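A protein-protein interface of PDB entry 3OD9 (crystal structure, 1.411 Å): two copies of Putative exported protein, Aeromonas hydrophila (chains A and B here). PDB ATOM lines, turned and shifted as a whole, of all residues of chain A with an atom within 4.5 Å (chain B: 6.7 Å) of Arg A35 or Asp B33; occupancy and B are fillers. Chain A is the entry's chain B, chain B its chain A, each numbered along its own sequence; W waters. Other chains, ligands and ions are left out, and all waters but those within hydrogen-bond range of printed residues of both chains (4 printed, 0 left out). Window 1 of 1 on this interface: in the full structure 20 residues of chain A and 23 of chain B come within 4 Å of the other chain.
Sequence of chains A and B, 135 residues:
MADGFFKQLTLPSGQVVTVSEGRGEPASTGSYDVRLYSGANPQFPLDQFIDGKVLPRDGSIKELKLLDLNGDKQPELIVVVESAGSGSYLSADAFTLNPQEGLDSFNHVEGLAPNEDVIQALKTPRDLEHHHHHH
Of the 17 printed residues of chain B, 8 touch a printed residue of chain A. Hydrophobic or aromatic side chains of chain B within 4 Å of the printed part of chain A: Val B54. Hydrophobic or aromatic side chains of chain A that line the printed part of chain B: Tyr A37 and Phe A49. Among the printed residues, Asp or Glu carboxylates within 4 Å of a Lys or Arg side-chain nitrogen of the other chain: Asp A33 with Arg B35 (3.0 Å) and Arg A35 with Asp B33 (3.0 Å).
Water W2 lies within hydrogen-bond range of OD1 of Asp A51 (2.8 Å), O of Val B54 (2.8 Å) and N of Gly A52 (3.5 Å). Water W3 lies within hydrogen-bond range of the backbone NH (N) of Arg B23 and the guanidinium group (NH1) of Arg A35. Water W1 lies within hydrogen-bond range of OG1 of Thr A18 (2.8 Å), OH of Tyr A37 (2.9 Å) and O of Arg B23 (2.9 Å). Water W4 bridges O of Gly A52 and N of Val B54.
Asp A33 touches Arg B35, and with the chains exchanged Arg A35 touches Asp B33. 5 positions are printed for both chains.
Printed residues of chain B within 4 Å of Arg A35: Ser B20 (3.9 Å), Gly B22 (3.7 Å), Ser B31 (2.7 Å), Tyr B32 (3.3 Å), Asp B33 (3.0 Å) and Val B54 (3.9 Å). Of the printed residues of chain B, Tyr A37 touches Glu B25 (2.6 Å). Printed residues of chain B within 4 Å of Phe A49: Ser B31 and Val B54. Printed residues of chain A within 4 Å of Ser B31: Arg A35 and Phe A49. Of the printed residues of chain A, Val B54 touches Arg A35, Phe A49 and Gly A52. The nearest printed residue of chain A that does not touch Asp B33 is Asp A33 (4.5 Å). The nearest printed residue of chain A that does not touch Val B54 is Asp A33 (4.5 Å).
The backbone NH of Thr B18 lies within hydrogen-bond range of the backbone carbonyl oxygen of Arg B35, 2.8 Å away. N of Gly B22 sits at hydrogen-bond distance from OE1 of Glu B25 (3.3 Å). The backbone NH (N) of Tyr B32 is in hydrogen-bond range of the backbone carbonyl oxygen (O) of Leu B55, 2.8 Å away. The guanidinium group (NH1) of Arg B35 lies within salt-bridge range of the side-chain carboxylate (OD2) of Asp B33, at 2.9 Å. N of Arg A35 sits at hydrogen-bond distance from O of Thr A18, 2.9 Å away. The side-chain carboxylate (OD2) of Asp A33 is in salt-bridge range of the guanidinium group (NH1) of Arg A35 (2.9 Å).
The side-chain hydroxyl of Tyr A37 sits at hydrogen-bond distance from the side-chain carboxylate of Glu B25 (2.6 Å). The side-chain hydroxyl (OG) of Ser B31 lies within hydrogen-bond range of the guanidinium group (NE) of Arg A35, at 2.7 Å. OD1 of Asp B33 lies within salt-bridge range of NH2 of Arg A35, 3.0 Å away. OD1 of Asp A33 is in salt-bridge range of NH2 of Arg B35 (3.0 Å).
Among the printed residues, merely in contact across the chains: Arg A35 with Tyr B32, Phe A49 with Ser B31, Phe A49 with Val B54, Arg A35 with Gly B22, Gly A52 with Val B54, Arg A35 with Val B54 and Arg A35 with Ser B20.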
ATOM      1  N   VAL A  16      38.522   3.939 -12.429  1.00  0.00           N
ATOM      2  CA  VAL A  16      38.325   2.512 -12.259  1.00  0.00           C
ATOM      3  C   VAL A  16      37.291   2.016 -13.250  1.00  0.00           C
ATOM      4  O   VAL A  16      36.264   2.655 -13.473  1.00  0.00           O
ATOM      5  CB  VAL A  16      37.862   2.193 -10.820  1.00  0.00           C
ATOM      6  CG1 VAL A  16      37.489   0.720 -10.666  1.00  0.00           C
ATOM      7  CG2 VAL A  16      38.957   2.595  -9.825  1.00  0.00           C
ATOM      8  N   VAL A  17      37.568   0.877 -13.864  1.00  0.00           N
ATOM      9  CA  VAL A  17      36.599   0.270 -14.759  1.00  0.00           C
ATOM     10  C   VAL A  17      36.378  -1.188 -14.378  1.00  0.00           C
ATOM     11  O   VAL A  17      37.303  -1.873 -13.967  1.00  0.00           O
ATOM     12  CB  VAL A  17      37.030   0.406 -16.250  1.00  0.00           C
ATOM     13  CG1 VAL A  17      38.321  -0.387 -16.541  1.00  0.00           C
ATOM     14  CG2 VAL A  17      35.906   0.003 -17.176  1.00  0.00           C
ATOM     15  N   THR A  18      35.134  -1.644 -14.471  1.00  0.00           N
ATOM     16  CA  THR A  18      34.864  -3.067 -14.313  1.00  0.00           C
ATOM     17  C   THR A  18      34.231  -3.577 -15.594  1.00  0.00           C
ATOM     18  O   THR A  18      33.529  -2.831 -16.291  1.00  0.00           O
ATOM     19  CB  THR A  18      33.944  -3.408 -13.117  1.00  0.00           C
ATOM     20  OG1 THR A  18      32.629  -2.894 -13.358  1.00  0.00           O
ATOM     21  CG2 THR A  18      34.503  -2.857 -11.802  1.00  0.00           C
ATOM     22  N   ASP A  33      29.216  -5.996 -19.938  1.00  0.00           N
ATOM     23  CA  ASP A  33      29.079  -4.570 -19.678  1.00  0.00           C
ATOM     24  C   ASP A  33      30.408  -3.994 -19.222  1.00  0.00           C
ATOM     25  O   ASP A  33      31.270  -4.719 -18.700  1.00  0.00           O
ATOM     26  CB  ASP A  33      27.947  -4.259 -18.689  1.00  0.00           C
ATOM     27  CG  ASP A  33      28.195  -4.819 -17.311  1.00  0.00           C
ATOM     28  OD1 ASP A  33      27.694  -5.925 -17.017  1.00  0.00           O
ATOM     29  OD2 ASP A  33      28.877  -4.134 -16.514  1.00  0.00           O
ATOM     30  N   VAL A  34      30.578  -2.702 -19.478  1.00  0.00           N
ATOM     31  CA  VAL A  34      31.723  -1.941 -19.011  1.00  0.00           C
ATOM     32  C   VAL A  34      31.164  -0.836 -18.136  1.00  0.00           C
ATOM     33  O   VAL A  34      30.261  -0.107 -18.557  1.00  0.00           O
ATOM     34  CB  VAL A  34      32.482  -1.302 -20.182  1.00  0.00           C
ATOM     35  CG1 VAL A  34      33.691  -0.525 -19.662  1.00  0.00           C
ATOM     36  CG2 VAL A  34      32.932  -2.392 -21.175  1.00  0.00           C
ATOM     37  N   ARG A  35      31.696  -0.709 -16.926  1.00  0.00           N
ATOM     38  CA  ARG A  35      31.274   0.349 -16.014  1.00  0.00           C
ATOM     39  C   ARG A  35      32.467   1.175 -15.581  1.00  0.00           C
ATOM     40  O   ARG A  35      33.491   0.629 -15.159  1.00  0.00           O
ATOM     41  CB  ARG A  35      30.581  -0.246 -14.791  1.00  0.00           C
ATOM     42  CG  ARG A  35      29.181  -0.799 -15.065  1.00  0.00           C
ATOM     43  CD  ARG A  35      28.700  -1.607 -13.867  1.00  0.00           C
ATOM     44  NE  ARG A  35      27.268  -1.552 -13.569  1.00  0.00           N
ATOM     45  CZ  ARG A  35      26.356  -2.437 -13.980  1.00  0.00           C
ATOM     46  NH1 ARG A  35      26.685  -3.442 -14.794  1.00  0.00           N
ATOM     47  NH2 ARG A  35      25.095  -2.299 -13.568  1.00  0.00           N
ATOM     48  N   LEU A  36      32.322   2.494 -15.666  1.00  0.00           N
ATOM     49  CA  LEU A  36      33.394   3.433 -15.358  1.00  0.00           C
ATOM     50  C   LEU A  36      33.053   4.166 -14.063  1.00  0.00           C
ATOM     51  O   LEU A  36      31.925   4.621 -13.894  1.00  0.00           O
ATOM     52  CB  LEU A  36      33.559   4.442 -16.504  1.00  0.00           C
ATOM     53  CG  LEU A  36      34.597   5.563 -16.343  1.00  0.00           C
ATOM     54  CD1 LEU A  36      36.007   4.980 -16.181  1.00  0.00           C
ATOM     55  CD2 LEU A  36      34.545   6.513 -17.521  1.00  0.00           C
ATOM     56  N   TYR A  37      34.039   4.276 -13.171  1.00  0.00           N
ATOM     57  CA  TYR A  37      33.912   4.951 -11.876  1.00  0.00           C
ATOM     58  C   TYR A  37      35.043   5.964 -11.756  1.00  0.00           C
ATOM     59  O   TYR A  37      36.080   5.806 -12.403  1.00  0.00           O
ATOM     60  CB  TYR A  37      34.030   3.947 -10.726  1.00  0.00           C
ATOM     61  CG  TYR A  37      33.028   2.825 -10.794  1.00  0.00           C
ATOM     62  CD1 TYR A  37      31.873   2.857 -10.016  1.00  0.00           C
ATOM     63  CD2 TYR A  37      33.233   1.725 -11.634  1.00  0.00           C
ATOM     64  CE1 TYR A  37      30.933   1.833 -10.069  1.00  0.00           C
ATOM     65  CE2 TYR A  37      32.298   0.685 -11.695  1.00  0.00           C
ATOM     66  CZ  TYR A  37      31.147   0.750 -10.911  1.00  0.00           C
ATOM     67  OH  TYR A  37      30.215  -0.255 -10.965  1.00  0.00           O
ATOM     68  N   PHE A  49      30.129   6.003  -9.401  1.00  0.00           N
ATOM     69  CA  PHE A  49      29.800   5.591 -10.757  1.00  0.00           C
ATOM     70  C   PHE A  49      29.679   6.789 -11.701  1.00  0.00           C
ATOM     71  O   PHE A  49      29.095   7.816 -11.341  1.00  0.00           O
ATOM     72  CB  PHE A  49      28.481   4.831 -10.738  1.00  0.00           C
ATOM     73  CG  PHE A  49      27.991   4.440 -12.093  1.00  0.00           C
ATOM     74  CD1 PHE A  49      28.620   3.430 -12.800  1.00  0.00           C
ATOM     75  CD2 PHE A  49      26.894   5.081 -12.663  1.00  0.00           C
ATOM     76  CE1 PHE A  49      28.173   3.061 -14.060  1.00  0.00           C
ATOM     77  CE2 PHE A  49      26.438   4.726 -13.923  1.00  0.00           C
ATOM     78  CZ  PHE A  49      27.078   3.703 -14.619  1.00  0.00           C
ATOM     79  N   ASP A  51      29.514   6.082 -15.696  1.00  0.00           N
ATOM     80  CA  ASP A  51      28.775   5.685 -16.888  1.00  0.00           C
ATOM     81  C   ASP A  51      29.038   4.219 -17.191  1.00  0.00           C
ATOM     82  O   ASP A  51      30.000   3.635 -16.671  1.00  0.00           O
ATOM     83  CB  ASP A  51      29.240   6.545 -18.055  1.00  0.00           C
ATOM     84  CG  ASP A  51      28.321   6.471 -19.267  1.00  0.00           C
ATOM     85  OD1 ASP A  51      27.152   6.041 -19.146  1.00  0.00           O
ATOM     86  OD2 ASP A  51      28.789   6.862 -20.359  1.00  0.00           O
ATOM     87  N   GLY A  52      28.187   3.621 -18.021  1.00  0.00           N
ATOM     88  CA  GLY A  52      28.357   2.232 -18.414  1.00  0.00           C
ATOM     89  C   GLY A  52      27.717   1.912 -19.749  1.00  0.00           C
ATOM     90  O   GLY A  52      26.844   2.637 -20.225  1.00  0.00           O
ATOM     91  N   THR B  18      16.465  -8.949 -17.505  1.00  0.00           N
ATOM     92  CA  THR B  18      17.104  -8.993 -16.191  1.00  0.00           C
ATOM     93  C   THR B  18      17.505  -7.600 -15.730  1.00  0.00           C
ATOM     94  O   THR B  18      17.792  -6.715 -16.544  1.00  0.00           O
ATOM     95  CB  THR B  18      18.321  -9.941 -16.138  1.00  0.00           C
ATOM     96  OG1 THR B  18      19.392  -9.395 -16.914  1.00  0.00           O
ATOM     97  CG2 THR B  18      17.945 -11.322 -16.658  1.00  0.00           C
ATOM     98  N   VAL B  19      17.510  -7.410 -14.419  1.00  0.00           N
ATOM     99  CA  VAL B  19      17.914  -6.141 -13.820  1.00  0.00           C
ATOM    100  C   VAL B  19      18.896  -6.448 -12.706  1.00  0.00           C
ATOM    101  O   VAL B  19      18.605  -7.281 -11.835  1.00  0.00           O
ATOM    102  CB  VAL B  19      16.705  -5.383 -13.232  1.00  0.00           C
ATOM    103  CG1 VAL B  19      17.134  -4.062 -12.643  1.00  0.00           C
ATOM    104  CG2 VAL B  19      15.647  -5.183 -14.311  1.00  0.00           C
ATOM    105  N   SER B  20      20.057  -5.794 -12.736  1.00  0.00           N
ATOM    106  CA  SER B  20      21.114  -6.031 -11.751  1.00  0.00           C
ATOM    107  C   SER B  20      21.659  -4.721 -11.234  1.00  0.00           C
ATOM    108  O   SER B  20      21.841  -3.778 -12.009  1.00  0.00           O
ATOM    109  CB  SER B  20      22.296  -6.767 -12.405  1.00  0.00           C
ATOM    110  OG  SER B  20      21.955  -8.081 -12.805  1.00  0.00           O
ATOM    111  N   GLU B  21      21.982  -4.658  -9.945  1.00  0.00           N
ATOM    112  CA  GLU B  21      22.813  -3.557  -9.465  1.00  0.00           C
ATOM    113  C   GLU B  21      24.288  -3.879  -9.778  1.00  0.00           C
ATOM    114  O   GLU B  21      24.654  -5.042  -9.934  1.00  0.00           O
ATOM    115  CB  GLU B  21      22.565  -3.289  -7.976  1.00  0.00           C
ATOM    116  CG  GLU B  21      21.200  -2.651  -7.728  1.00  0.00           C
ATOM    117  CD  GLU B  21      20.888  -2.355  -6.265  1.00  0.00           C
ATOM    118  OE1 GLU B  21      21.618  -2.820  -5.362  1.00  0.00           O
ATOM    119  OE2 GLU B  21      19.880  -1.657  -6.018  1.00  0.00           O
ATOM    120  N   GLY B  22      25.119  -2.850  -9.917  1.00  0.00           N
ATOM    121  CA  GLY B  22      26.522  -3.057 -10.242  1.00  0.00           C
ATOM    122  C   GLY B  22      27.262  -3.900  -9.211  1.00  0.00           C
ATOM    123  O   GLY B  22      27.113  -3.717  -7.993  1.00  0.00           O
ATOM    124  N   ARG B  23      28.079  -4.834  -9.690  1.00  0.00           N
ATOM    125  CA  ARG B  23      28.830  -5.705  -8.790  1.00  0.00           C
ATOM    126  C   ARG B  23      29.880  -4.948  -7.976  1.00  0.00           C
ATOM    127  O   ARG B  23      30.636  -4.133  -8.515  1.00  0.00           O
ATOM    128  CB  ARG B  23      29.497  -6.840  -9.567  1.00  0.00           C
ATOM    129  CG  ARG B  23      30.316  -7.756  -8.698  1.00  0.00           C
ATOM    130  CD  ARG B  23      30.674  -9.049  -9.410  1.00  0.00           C
ATOM    131  NE  ARG B  23      31.642  -9.820  -8.634  1.00  0.00           N
ATOM    132  CZ  ARG B  23      32.073 -11.034  -8.962  1.00  0.00           C
ATOM    133  NH1 ARG B  23      31.625 -11.623 -10.059  1.00  0.00           N
ATOM    134  NH2 ARG B  23      32.959 -11.655  -8.195  1.00  0.00           N
ATOM    135  N   GLU B  25      29.444  -2.658  -5.777  1.00  0.00           N
ATOM    136  CA  GLU B  25      29.037  -1.297  -5.430  1.00  0.00           C
ATOM    137  C   GLU B  25      28.439  -1.210  -4.027  1.00  0.00           C
ATOM    138  O   GLU B  25      27.942  -2.200  -3.492  1.00  0.00           O
ATOM    139  CB  GLU B  25      28.012  -0.782  -6.442  1.00  0.00           C
ATOM    140  CG  GLU B  25      28.544  -0.621  -7.851  1.00  0.00           C
ATOM    141  CD  GLU B  25      27.483  -0.155  -8.820  1.00  0.00           C
ATOM    142  OE1 GLU B  25      26.282  -0.149  -8.446  1.00  0.00           O
ATOM    143  OE2 GLU B  25      27.849   0.214  -9.955  1.00  0.00           O
ATOM    144  N   SER B  31      25.025   1.986  -9.744  1.00  0.00           N
ATOM    145  CA  SER B  31      24.409   1.811 -11.045  1.00  0.00           C
ATOM    146  C   SER B  31      23.509   0.590 -11.036  1.00  0.00           C
ATOM    147  O   SER B  31      23.526  -0.231 -10.101  1.00  0.00           O
ATOM    148  CB  SER B  31      25.487   1.594 -12.109  1.00  0.00           C
ATOM    149  OG  SER B  31      26.124   0.322 -11.937  1.00  0.00           O
ATOM    150  N   TYR B  32      22.742   0.450 -12.100  1.00  0.00           N
ATOM    151  CA  TYR B  32      22.091  -0.824 -12.372  1.00  0.00           C
ATOM    152  C   TYR B  32      22.046  -0.999 -13.873  1.00  0.00           C
ATOM    153  O   TYR B  32      22.237  -0.039 -14.626  1.00  0.00           O
ATOM    154  CB  TYR B  32      20.685  -0.890 -11.755  1.00  0.00           C
ATOM    155  CG  TYR B  32      19.666   0.006 -12.413  1.00  0.00           C
ATOM    156  CD1 TYR B  32      18.865  -0.460 -13.447  1.00  0.00           C
ATOM    157  CD2 TYR B  32      19.493   1.328 -11.996  1.00  0.00           C
ATOM    158  CE1 TYR B  32      17.919   0.360 -14.043  1.00  0.00           C
ATOM    159  CE2 TYR B  32      18.549   2.143 -12.580  1.00  0.00           C
ATOM    160  CZ  TYR B  32      17.769   1.661 -13.607  1.00  0.00           C
ATOM    161  OH  TYR B  32      16.839   2.476 -14.202  1.00  0.00           O
ATOM    162  N   ASP B  33      21.841  -2.230 -14.323  1.00  0.00           N
ATOM    163  CA  ASP B  33      21.659  -2.453 -15.742  1.00  0.00           C
ATOM    164  C   ASP B  33      20.380  -3.212 -15.996  1.00  0.00           C
ATOM    165  O   ASP B  33      19.865  -3.919 -15.116  1.00  0.00           O
ATOM    166  CB  ASP B  33      22.862  -3.160 -16.380  1.00  0.00           C
ATOM    167  CG  ASP B  33      23.090  -4.552 -15.837  1.00  0.00           C
ATOM    168  OD1 ASP B  33      23.887  -4.696 -14.885  1.00  0.00           O
ATOM    169  OD2 ASP B  33      22.492  -5.501 -16.371  1.00  0.00           O
ATOM    170  N   VAL B  34      19.874  -3.030 -17.208  1.00  0.00           N
ATOM    171  CA  VAL B  34      18.698  -3.714 -17.716  1.00  0.00           C
ATOM    172  C   VAL B  34      19.157  -4.426 -18.979  1.00  0.00           C
ATOM    173  O   VAL B  34      19.730  -3.796 -19.865  1.00  0.00           O
ATOM    174  CB  VAL B  34      17.583  -2.708 -18.077  1.00  0.00           C
ATOM    175  CG1 VAL B  34      16.403  -3.409 -18.721  1.00  0.00           C
ATOM    176  CG2 VAL B  34      17.135  -1.936 -16.837  1.00  0.00           C
ATOM    177  N   ARG B  35      18.900  -5.728 -19.058  1.00  0.00           N
ATOM    178  CA  ARG B  35      19.276  -6.539 -20.212  1.00  0.00           C
ATOM    179  C   ARG B  35      18.064  -7.273 -20.761  1.00  0.00           C
ATOM    180  O   ARG B  35      17.321  -7.911 -20.008  1.00  0.00           O
ATOM    181  CB  ARG B  35      20.368  -7.545 -19.825  1.00  0.00           C
ATOM    182  CG  ARG B  35      21.762  -6.941 -19.622  1.00  0.00           C
ATOM    183  CD  ARG B  35      22.684  -7.959 -18.977  1.00  0.00           C
ATOM    184  NE  ARG B  35      24.087  -7.905 -19.396  1.00  0.00           N
ATOM    185  CZ  ARG B  35      25.067  -7.322 -18.720  1.00  0.00           C
ATOM    186  NH1 ARG B  35      24.813  -6.614 -17.616  1.00  0.00           N
ATOM    187  NH2 ARG B  35      26.306  -7.411 -19.183  1.00  0.00           N
ATOM    188  N   GLY B  52      21.143  -3.968 -23.928  1.00  0.00           N
ATOM    189  CA  GLY B  52      21.102  -3.588 -22.530  1.00  0.00           C
ATOM    190  C   GLY B  52      21.515  -2.147 -22.326  1.00  0.00           C
ATOM    191  O   GLY B  52      22.114  -1.520 -23.212  1.00  0.00           O
ATOM    192  N   LYS B  53      21.218  -1.625 -21.143  1.00  0.00           N
ATOM    193  CA  LYS B  53      21.592  -0.268 -20.767  1.00  0.00           C
ATOM    194  C   LYS B  53      22.102  -0.253 -19.332  1.00  0.00           C
ATOM    195  O   LYS B  53      21.639  -1.043 -18.507  1.00  0.00           O
ATOM    196  CB  LYS B  53      20.378   0.647 -20.861  1.00  0.00           C
ATOM    197  CG  LYS B  53      19.844   0.889 -22.261  1.00  0.00           C
ATOM    198  CD  LYS B  53      18.633   1.815 -22.192  1.00  0.00           C
ATOM    199  CE  LYS B  53      18.092   2.164 -23.566  1.00  0.00           C
ATOM    200  NZ  LYS B  53      19.103   2.897 -24.391  1.00  0.00           N
ATOM    201  N   VAL B  54      23.026   0.658 -19.031  1.00  0.00           N
ATOM    202  CA  VAL B  54      23.480   0.866 -17.658  1.00  0.00           C
ATOM    203  C   VAL B  54      23.074   2.270 -17.249  1.00  0.00           C
ATOM    204  O   VAL B  54      23.296   3.219 -18.003  1.00  0.00           O
ATOM    205  CB  VAL B  54      25.002   0.739 -17.510  1.00  0.00           C
ATOM    206  CG1 VAL B  54      25.398   0.789 -16.037  1.00  0.00           C
ATOM    207  CG2 VAL B  54      25.487  -0.553 -18.129  1.00  0.00           C
ATOM    208  N   LEU B  55      22.488   2.394 -16.059  1.00  0.00           N
ATOM    209  CA  LEU B  55      21.983   3.671 -15.550  1.00  0.00           C
ATOM    210  C   LEU B  55      22.482   3.920 -14.129  1.00  0.00           C
ATOM    211  O   LEU B  55      22.722   2.978 -13.381  1.00  0.00           O
ATOM    212  CB  LEU B  55      20.448   3.685 -15.554  1.00  0.00           C
ATOM    213  CG  LEU B  55      19.796   3.716 -16.935  1.00  0.00           C
ATOM    214  CD1 LEU B  55      19.696   2.293 -17.489  1.00  0.00           C
ATOM    215  CD2 LEU B  55      18.453   4.390 -16.902  1.00  0.00           C
ATOM    216  N   ILE B  61      17.457  -0.124  -5.600  1.00  0.00           N
ATOM    217  CA  ILE B  61      16.241  -0.513  -6.300  1.00  0.00           C
ATOM    218  C   ILE B  61      15.233  -1.010  -5.275  1.00  0.00           C
ATOM    219  O   ILE B  61      15.547  -1.867  -4.440  1.00  0.00           O
ATOM    220  CB  ILE B  61      16.500  -1.593  -7.366  1.00  0.00           C
ATOM    221  CG1 ILE B  61      17.333  -0.998  -8.510  1.00  0.00           C
ATOM    222  CG2 ILE B  61      15.174  -2.164  -7.885  1.00  0.00           C
ATOM    223  CD1 ILE B  61      17.796  -2.011  -9.525  1.00  0.00           C
HETATM  224  O   HOH W   1      30.894  -3.024 -11.146  1.00  0.00           O
HETATM  225  O   HOH W   2      25.190   5.219 -17.365  1.00  0.00           O
HETATM  226  O   HOH W   3      28.631  -4.818 -12.417  1.00  0.00           O
HETATM  227  O   HOH W   4      24.226   2.055 -21.246  1.00  0.00           O
